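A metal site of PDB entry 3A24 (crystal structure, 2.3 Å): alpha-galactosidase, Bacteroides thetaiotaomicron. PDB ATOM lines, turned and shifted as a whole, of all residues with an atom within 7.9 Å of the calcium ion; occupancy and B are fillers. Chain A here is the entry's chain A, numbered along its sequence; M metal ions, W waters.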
ATOM      1  N   SER A 151     -16.977  11.225 -30.725  1.00  0.00           N
ATOM      2  CA  SER A 151     -17.617   9.911 -30.700  1.00  0.00           C
ATOM      3  C   SER A 151     -17.717   9.221 -32.040  1.00  0.00           C
ATOM      4  O   SER A 151     -18.006   8.018 -32.100  1.00  0.00           O
ATOM      5  CB  SER A 151     -19.049  10.031 -30.144  1.00  0.00           C
ATOM      6  OG  SER A 151     -19.061  10.523 -28.821  1.00  0.00           O
ATOM      7  N   GLU A 153     -19.997   9.647 -34.064  1.00  0.00           N
ATOM      8  CA  GLU A 153     -21.427   9.353 -34.158  1.00  0.00           C
ATOM      9  C   GLU A 153     -22.132  10.562 -34.761  1.00  0.00           C
ATOM     10  O   GLU A 153     -22.262  11.585 -34.101  1.00  0.00           O
ATOM     11  CB  GLU A 153     -22.011   9.074 -32.764  1.00  0.00           C
ATOM     12  CG  GLU A 153     -21.209   8.096 -31.906  1.00  0.00           C
ATOM     13  CD  GLU A 153     -21.763   7.949 -30.487  1.00  0.00           C
ATOM     14  OE1 GLU A 153     -22.104   8.983 -29.870  1.00  0.00           O
ATOM     15  OE2 GLU A 153     -21.842   6.807 -29.986  1.00  0.00           O
ATOM     16  N   TRP A 289     -30.616  -6.627 -23.923  1.00  0.00           N
ATOM     17  CA  TRP A 289     -29.993  -5.417 -23.418  1.00  0.00           C
ATOM     18  C   TRP A 289     -30.775  -4.715 -22.322  1.00  0.00           C
ATOM     19  O   TRP A 289     -31.997  -4.821 -22.225  1.00  0.00           O
ATOM     20  CB  TRP A 289     -29.699  -4.466 -24.585  1.00  0.00           C
ATOM     21  CG  TRP A 289     -28.624  -3.453 -24.293  1.00  0.00           C
ATOM     22  CD1 TRP A 289     -27.634  -3.555 -23.358  1.00  0.00           C
ATOM     23  CD2 TRP A 289     -28.428  -2.200 -24.957  1.00  0.00           C
ATOM     24  NE1 TRP A 289     -26.836  -2.439 -23.389  1.00  0.00           N
ATOM     25  CE2 TRP A 289     -27.299  -1.592 -24.361  1.00  0.00           C
ATOM     26  CE3 TRP A 289     -29.087  -1.532 -26.001  1.00  0.00           C
ATOM     27  CZ2 TRP A 289     -26.819  -0.339 -24.769  1.00  0.00           C
ATOM     28  CZ3 TRP A 289     -28.614  -0.285 -26.405  1.00  0.00           C
ATOM     29  CH2 TRP A 289     -27.485   0.302 -25.787  1.00  0.00           C
ATOM     30  N   TRP A 291     -29.575  -1.168 -20.888  1.00  0.00           N
ATOM     31  CA  TRP A 291     -29.443   0.285 -20.957  1.00  0.00           C
ATOM     32  C   TRP A 291     -30.417   1.097 -21.820  1.00  0.00           C
ATOM     33  O   TRP A 291     -31.016   2.047 -21.328  1.00  0.00           O
ATOM     34  CB  TRP A 291     -28.007   0.630 -21.367  1.00  0.00           C
ATOM     35  CG  TRP A 291     -27.653   2.045 -21.115  1.00  0.00           C
ATOM     36  CD1 TRP A 291     -27.292   2.608 -19.926  1.00  0.00           C
ATOM     37  CD2 TRP A 291     -27.623   3.105 -22.085  1.00  0.00           C
ATOM     38  NE1 TRP A 291     -27.044   3.945 -20.088  1.00  0.00           N
ATOM     39  CE2 TRP A 291     -27.243   4.282 -21.402  1.00  0.00           C
ATOM     40  CE3 TRP A 291     -27.893   3.173 -23.453  1.00  0.00           C
ATOM     41  CZ2 TRP A 291     -27.111   5.511 -22.042  1.00  0.00           C
ATOM     42  CZ3 TRP A 291     -27.762   4.402 -24.094  1.00  0.00           C
ATOM     43  CH2 TRP A 291     -27.376   5.550 -23.392  1.00  0.00           C
ATOM     44  N   TRP A 366     -19.730  -4.048 -19.297  1.00  0.00           N
ATOM     45  CA  TRP A 366     -19.439  -2.758 -19.908  1.00  0.00           C
ATOM     46  C   TRP A 366     -18.311  -2.141 -19.082  1.00  0.00           C
ATOM     47  O   TRP A 366     -18.269  -2.307 -17.856  1.00  0.00           O
ATOM     48  CB  TRP A 366     -20.655  -1.847 -19.843  1.00  0.00           C
ATOM     49  CG  TRP A 366     -20.462  -0.482 -20.419  1.00  0.00           C
ATOM     50  CD1 TRP A 366     -20.783  -0.065 -21.685  1.00  0.00           C
ATOM     51  CD2 TRP A 366     -19.926   0.669 -19.743  1.00  0.00           C
ATOM     52  NE1 TRP A 366     -20.489   1.272 -21.838  1.00  0.00           N
ATOM     53  CE2 TRP A 366     -19.969   1.751 -20.660  1.00  0.00           C
ATOM     54  CE3 TRP A 366     -19.431   0.892 -18.451  1.00  0.00           C
ATOM     55  CZ2 TRP A 366     -19.534   3.034 -20.323  1.00  0.00           C
ATOM     56  CZ3 TRP A 366     -18.995   2.175 -18.113  1.00  0.00           C
ATOM     57  CH2 TRP A 366     -19.045   3.235 -19.050  1.00  0.00           C
ATOM     58  N   LYS A 392     -17.582  -4.804 -23.138  1.00  0.00           N
ATOM     59  CA  LYS A 392     -18.083  -3.761 -24.010  1.00  0.00           C
ATOM     60  C   LYS A 392     -17.317  -2.539 -23.503  1.00  0.00           C
ATOM     61  O   LYS A 392     -17.676  -1.958 -22.476  1.00  0.00           O
ATOM     62  CB  LYS A 392     -19.592  -3.564 -23.808  1.00  0.00           C
ATOM     63  CG  LYS A 392     -20.177  -2.435 -24.652  1.00  0.00           C
ATOM     64  CD  LYS A 392     -21.655  -2.219 -24.386  1.00  0.00           C
ATOM     65  CE  LYS A 392     -22.189  -1.031 -25.175  1.00  0.00           C
ATOM     66  NZ  LYS A 392     -23.620  -0.750 -24.875  1.00  0.00           N
ATOM     67  N   ASP A 394     -16.206   1.229 -23.735  1.00  0.00           N
ATOM     68  CA  ASP A 394     -16.771   2.462 -24.242  1.00  0.00           C
ATOM     69  C   ASP A 394     -15.984   3.738 -23.905  1.00  0.00           C
ATOM     70  O   ASP A 394     -15.106   3.731 -23.041  1.00  0.00           O
ATOM     71  CB  ASP A 394     -18.201   2.567 -23.677  1.00  0.00           C
ATOM     72  CG  ASP A 394     -19.141   3.374 -24.536  1.00  0.00           C
ATOM     73  OD1 ASP A 394     -20.363   3.304 -24.276  1.00  0.00           O
ATOM     74  OD2 ASP A 394     -18.682   4.086 -25.462  1.00  0.00           O
ATOM     75  N   PHE A 395     -16.323   4.805 -24.614  1.00  0.00           N
ATOM     76  CA  PHE A 395     -15.759   6.146 -24.447  1.00  0.00           C
ATOM     77  C   PHE A 395     -14.308   6.448 -24.787  1.00  0.00           C
ATOM     78  O   PHE A 395     -13.699   7.321 -24.165  1.00  0.00           O
ATOM     79  CB  PHE A 395     -16.072   6.656 -23.037  1.00  0.00           C
ATOM     80  CG  PHE A 395     -17.527   6.972 -22.835  1.00  0.00           C
ATOM     81  CD1 PHE A 395     -18.401   6.009 -22.332  1.00  0.00           C
ATOM     82  CD2 PHE A 395     -18.049   8.212 -23.195  1.00  0.00           C
ATOM     83  CE1 PHE A 395     -19.763   6.273 -22.197  1.00  0.00           C
ATOM     84  CE2 PHE A 395     -19.401   8.495 -23.063  1.00  0.00           C
ATOM     85  CZ  PHE A 395     -20.270   7.524 -22.563  1.00  0.00           C
ATOM     86  N   ASP A 397     -13.336   7.723 -27.661  1.00  0.00           N
ATOM     87  CA  ASP A 397     -13.492   9.035 -28.299  1.00  0.00           C
ATOM     88  C   ASP A 397     -12.232   9.629 -28.930  1.00  0.00           C
ATOM     89  O   ASP A 397     -12.117  10.852 -29.070  1.00  0.00           O
ATOM     90  CB  ASP A 397     -14.071  10.030 -27.289  1.00  0.00           C
ATOM     91  CG  ASP A 397     -15.537   9.765 -26.974  1.00  0.00           C
ATOM     92  OD1 ASP A 397     -16.006   8.635 -27.217  1.00  0.00           O
ATOM     93  OD2 ASP A 397     -16.220  10.679 -26.460  1.00  0.00           O
ATOM     94  N   HIS A 424     -17.324   0.548 -28.240  1.00  0.00           N
ATOM     95  CA  HIS A 424     -18.224   1.679 -28.373  1.00  0.00           C
ATOM     96  C   HIS A 424     -17.456   2.975 -28.149  1.00  0.00           C
ATOM     97  O   HIS A 424     -16.371   2.950 -27.583  1.00  0.00           O
ATOM     98  CB  HIS A 424     -19.386   1.593 -27.370  1.00  0.00           C
ATOM     99  CG  HIS A 424     -20.532   0.771 -27.853  1.00  0.00           C
ATOM    100  ND1 HIS A 424     -21.837   1.168 -27.719  1.00  0.00           N
ATOM    101  CD2 HIS A 424     -20.570  -0.431 -28.474  1.00  0.00           C
ATOM    102  CE1 HIS A 424     -22.635   0.252 -28.238  1.00  0.00           C
ATOM    103  NE2 HIS A 424     -21.898  -0.733 -28.706  1.00  0.00           N
ATOM    104  N   GLY A 425     -18.017   4.089 -28.596  1.00  0.00           N
ATOM    105  CA  GLY A 425     -17.329   5.352 -28.445  1.00  0.00           C
ATOM    106  C   GLY A 425     -16.046   5.225 -29.250  1.00  0.00           C
ATOM    107  O   GLY A 425     -14.973   5.663 -28.815  1.00  0.00           O
ATOM    108  N   THR A 426     -16.169   4.617 -30.424  1.00  0.00           N
ATOM    109  CA  THR A 426     -15.022   4.402 -31.309  1.00  0.00           C
ATOM    110  C   THR A 426     -15.358   4.786 -32.739  1.00  0.00           C
ATOM    111  O   THR A 426     -16.457   5.262 -33.023  1.00  0.00           O
ATOM    112  CB  THR A 426     -14.578   2.911 -31.284  1.00  0.00           C
ATOM    113  OG1 THR A 426     -13.386   2.764 -32.053  1.00  0.00           O
ATOM    114  CG2 THR A 426     -15.663   2.031 -31.873  1.00  0.00           C
ATOM    115  N   GLU A 443     -19.067   0.377 -32.591  1.00  0.00           N
ATOM    116  CA  GLU A 443     -20.092   1.402 -32.649  1.00  0.00           C
ATOM    117  C   GLU A 443     -19.719   2.380 -33.756  1.00  0.00           C
ATOM    118  O   GLU A 443     -19.689   1.998 -34.923  1.00  0.00           O
ATOM    119  CB  GLU A 443     -20.238   2.140 -31.308  1.00  0.00           C
ATOM    120  CG  GLU A 443     -21.604   2.827 -31.160  1.00  0.00           C
ATOM    121  CD  GLU A 443     -21.774   3.575 -29.852  1.00  0.00           C
ATOM    122  OE1 GLU A 443     -22.938   3.843 -29.482  1.00  0.00           O
ATOM    123  OE2 GLU A 443     -20.771   3.911 -29.200  1.00  0.00           O
ATOM    124  N   GLY A 444     -19.428   3.636 -33.419  1.00  0.00           N
ATOM    125  CA  GLY A 444     -19.084   4.593 -34.453  1.00  0.00           C
ATOM    126  C   GLY A 444     -20.241   4.692 -35.422  1.00  0.00           C
ATOM    127  O   GLY A 444     -20.060   4.699 -36.653  1.00  0.00           O
ATOM    128  N   VAL A 445     -21.442   4.781 -34.869  1.00  0.00           N
ATOM    129  CA  VAL A 445     -22.661   4.883 -35.654  1.00  0.00           C
ATOM    130  C   VAL A 445     -23.695   5.630 -34.818  1.00  0.00           C
ATOM    131  O   VAL A 445     -23.746   5.473 -33.597  1.00  0.00           O
ATOM    132  CB  VAL A 445     -23.190   3.478 -36.015  1.00  0.00           C
ATOM    133  CG1 VAL A 445     -23.481   2.687 -34.751  1.00  0.00           C
ATOM    134  CG2 VAL A 445     -24.423   3.579 -36.885  1.00  0.00           C
ATOM    135  N   ASN A 446     -24.503   6.468 -35.451  1.00  0.00           N
ATOM    136  CA  ASN A 446     -25.518   7.222 -34.727  1.00  0.00           C
ATOM    137  C   ASN A 446     -26.733   6.310 -34.513  1.00  0.00           C
ATOM    138  O   ASN A 446     -27.776   6.483 -35.141  1.00  0.00           O
ATOM    139  CB  ASN A 446     -25.905   8.471 -35.538  1.00  0.00           C
ATOM    140  CG  ASN A 446     -26.067   9.701 -34.667  1.00  0.00           C
ATOM    141  OD1 ASN A 446     -25.224   9.985 -33.815  1.00  0.00           O
ATOM    142  ND2 ASN A 446     -27.147  10.449 -34.891  1.00  0.00           N
ATOM    143  N   GLY A 447     -26.558   5.350 -33.606  1.00  0.00           N
ATOM    144  CA  GLY A 447     -27.579   4.352 -33.309  1.00  0.00           C
ATOM    145  C   GLY A 447     -28.857   4.768 -32.606  1.00  0.00           C
ATOM    146  O   GLY A 447     -29.079   5.949 -32.310  1.00  0.00           O
ATOM    147  N   GLU A 449     -29.740   4.634 -29.701  1.00  0.00           N
ATOM    148  CA  GLU A 449     -29.589   5.258 -28.393  1.00  0.00           C
ATOM    149  C   GLU A 449     -29.886   6.742 -28.521  1.00  0.00           C
ATOM    150  O   GLU A 449     -30.273   7.403 -27.555  1.00  0.00           O
ATOM    151  CB  GLU A 449     -28.164   5.055 -27.852  1.00  0.00           C
ATOM    152  CG  GLU A 449     -27.093   5.936 -28.503  1.00  0.00           C
ATOM    153  CD  GLU A 449     -25.733   5.828 -27.829  1.00  0.00           C
ATOM    154  OE1 GLU A 449     -25.684   5.684 -26.583  1.00  0.00           O
ATOM    155  OE2 GLU A 449     -24.701   5.904 -28.533  1.00  0.00           O
ATOM    156  N   GLN A 450     -29.711   7.281 -29.734  1.00  0.00           N
ATOM    157  CA  GLN A 450     -29.961   8.694 -30.018  1.00  0.00           C
ATOM    158  C   GLN A 450     -31.433   9.042 -29.828  1.00  0.00           C
ATOM    159  O   GLN A 450     -31.779  10.212 -29.602  1.00  0.00           O
ATOM    160  CB  GLN A 450     -29.529   9.032 -31.452  1.00  0.00           C
ATOM    161  CG  GLN A 450     -28.037   8.877 -31.757  1.00  0.00           C
ATOM    162  CD  GLN A 450     -27.159   9.779 -30.916  1.00  0.00           C
ATOM    163  OE1 GLN A 450     -27.486  10.939 -30.667  1.00  0.00           O
ATOM    164  NE2 GLN A 450     -26.025   9.247 -30.460  1.00  0.00           N
ATOM    165  N   TRP A 453     -32.717  10.995 -26.599  1.00  0.00           N
ATOM    166  CA  TRP A 453     -32.564  12.428 -26.361  1.00  0.00           C
ATOM    167  C   TRP A 453     -32.628  13.350 -27.572  1.00  0.00           C
ATOM    168  O   TRP A 453     -32.764  14.568 -27.425  1.00  0.00           O
ATOM    169  CB  TRP A 453     -31.227  12.655 -25.635  1.00  0.00           C
ATOM    170  CG  TRP A 453     -30.088  12.025 -26.353  1.00  0.00           C
ATOM    171  CD1 TRP A 453     -29.562  12.406 -27.562  1.00  0.00           C
ATOM    172  CD2 TRP A 453     -29.353  10.860 -25.947  1.00  0.00           C
ATOM    173  NE1 TRP A 453     -28.556  11.547 -27.931  1.00  0.00           N
ATOM    174  CE2 TRP A 453     -28.394  10.591 -26.959  1.00  0.00           C
ATOM    175  CE3 TRP A 453     -29.406  10.025 -24.828  1.00  0.00           C
ATOM    176  CZ2 TRP A 453     -27.509   9.511 -26.884  1.00  0.00           C
ATOM    177  CZ3 TRP A 453     -28.521   8.944 -24.753  1.00  0.00           C
ATOM    178  CH2 TRP A 453     -27.579   8.707 -25.776  1.00  0.00           C
ATOM    179  N   ASP A 478     -22.877  -1.783 -34.174  1.00  0.00           N
ATOM    180  CA  ASP A 478     -23.663  -2.124 -33.002  1.00  0.00           C
ATOM    181  C   ASP A 478     -24.673  -0.974 -32.913  1.00  0.00           C
ATOM    182  O   ASP A 478     -24.550  -0.078 -32.068  1.00  0.00           O
ATOM    183  CB  ASP A 478     -22.793  -2.193 -31.736  1.00  0.00           C
ATOM    184  CG  ASP A 478     -23.527  -2.837 -30.563  1.00  0.00           C
ATOM    185  OD1 ASP A 478     -22.980  -2.888 -29.439  1.00  0.00           O
ATOM    186  OD2 ASP A 478     -24.671  -3.297 -30.766  1.00  0.00           O
HETATM  187 CA    CA M   1     -22.392   5.742 -27.848  1.00  0.00          CA
HETATM  188  O   HOH W   1     -22.318   3.676 -26.506  1.00  0.00           O
HETATM  189  O   HOH W   2     -20.137   5.916 -26.684  1.00  0.00           O
HETATM  190  O   HOH W   3     -23.487   6.374 -25.120  1.00  0.00           O
HETATM  191  O   HOH W   4     -22.475   8.241 -27.198  1.00  0.00           O
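The backbone carbonyl oxygen of Glu 153 lies close to the side-chain amide oxygen of Asn 446 (3.4 Å). The side-chain carboxylate (OE2) of Glu 443 sits close to a ring nitrogen (ND1) of His 424 (3.3 Å). The backbone NH (N) of Gly 425 sits close to the side-chain carboxylate (OE2) of Glu 443 (2.8 Å).
Three residues have an atom within 4 Å of the calcium ion: Glu 153, Glu 443 and Glu 449.
The calcium ion is bound by OE2 of Glu 449 (2.4 Å), OE2 of Glu 153 (2.5 Å), water W1 (2.5 Å), water W2 (2.5 Å), OE1 of Glu 443 (2.6 Å), water W4 (2.6 Å) and OE2 of Glu 443 (2.8 Å). Slightly farther from the calcium ion lies water W3 (3.0 Å).
Water W1 lies within hydrogen-bond range of ND1 of His 424 (2.8 Å) and OD1 of Asp 394 (3.0 Å). Water W2 lies within hydrogen-bond range of OD2 of Asp 394 and N of Gly 425.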
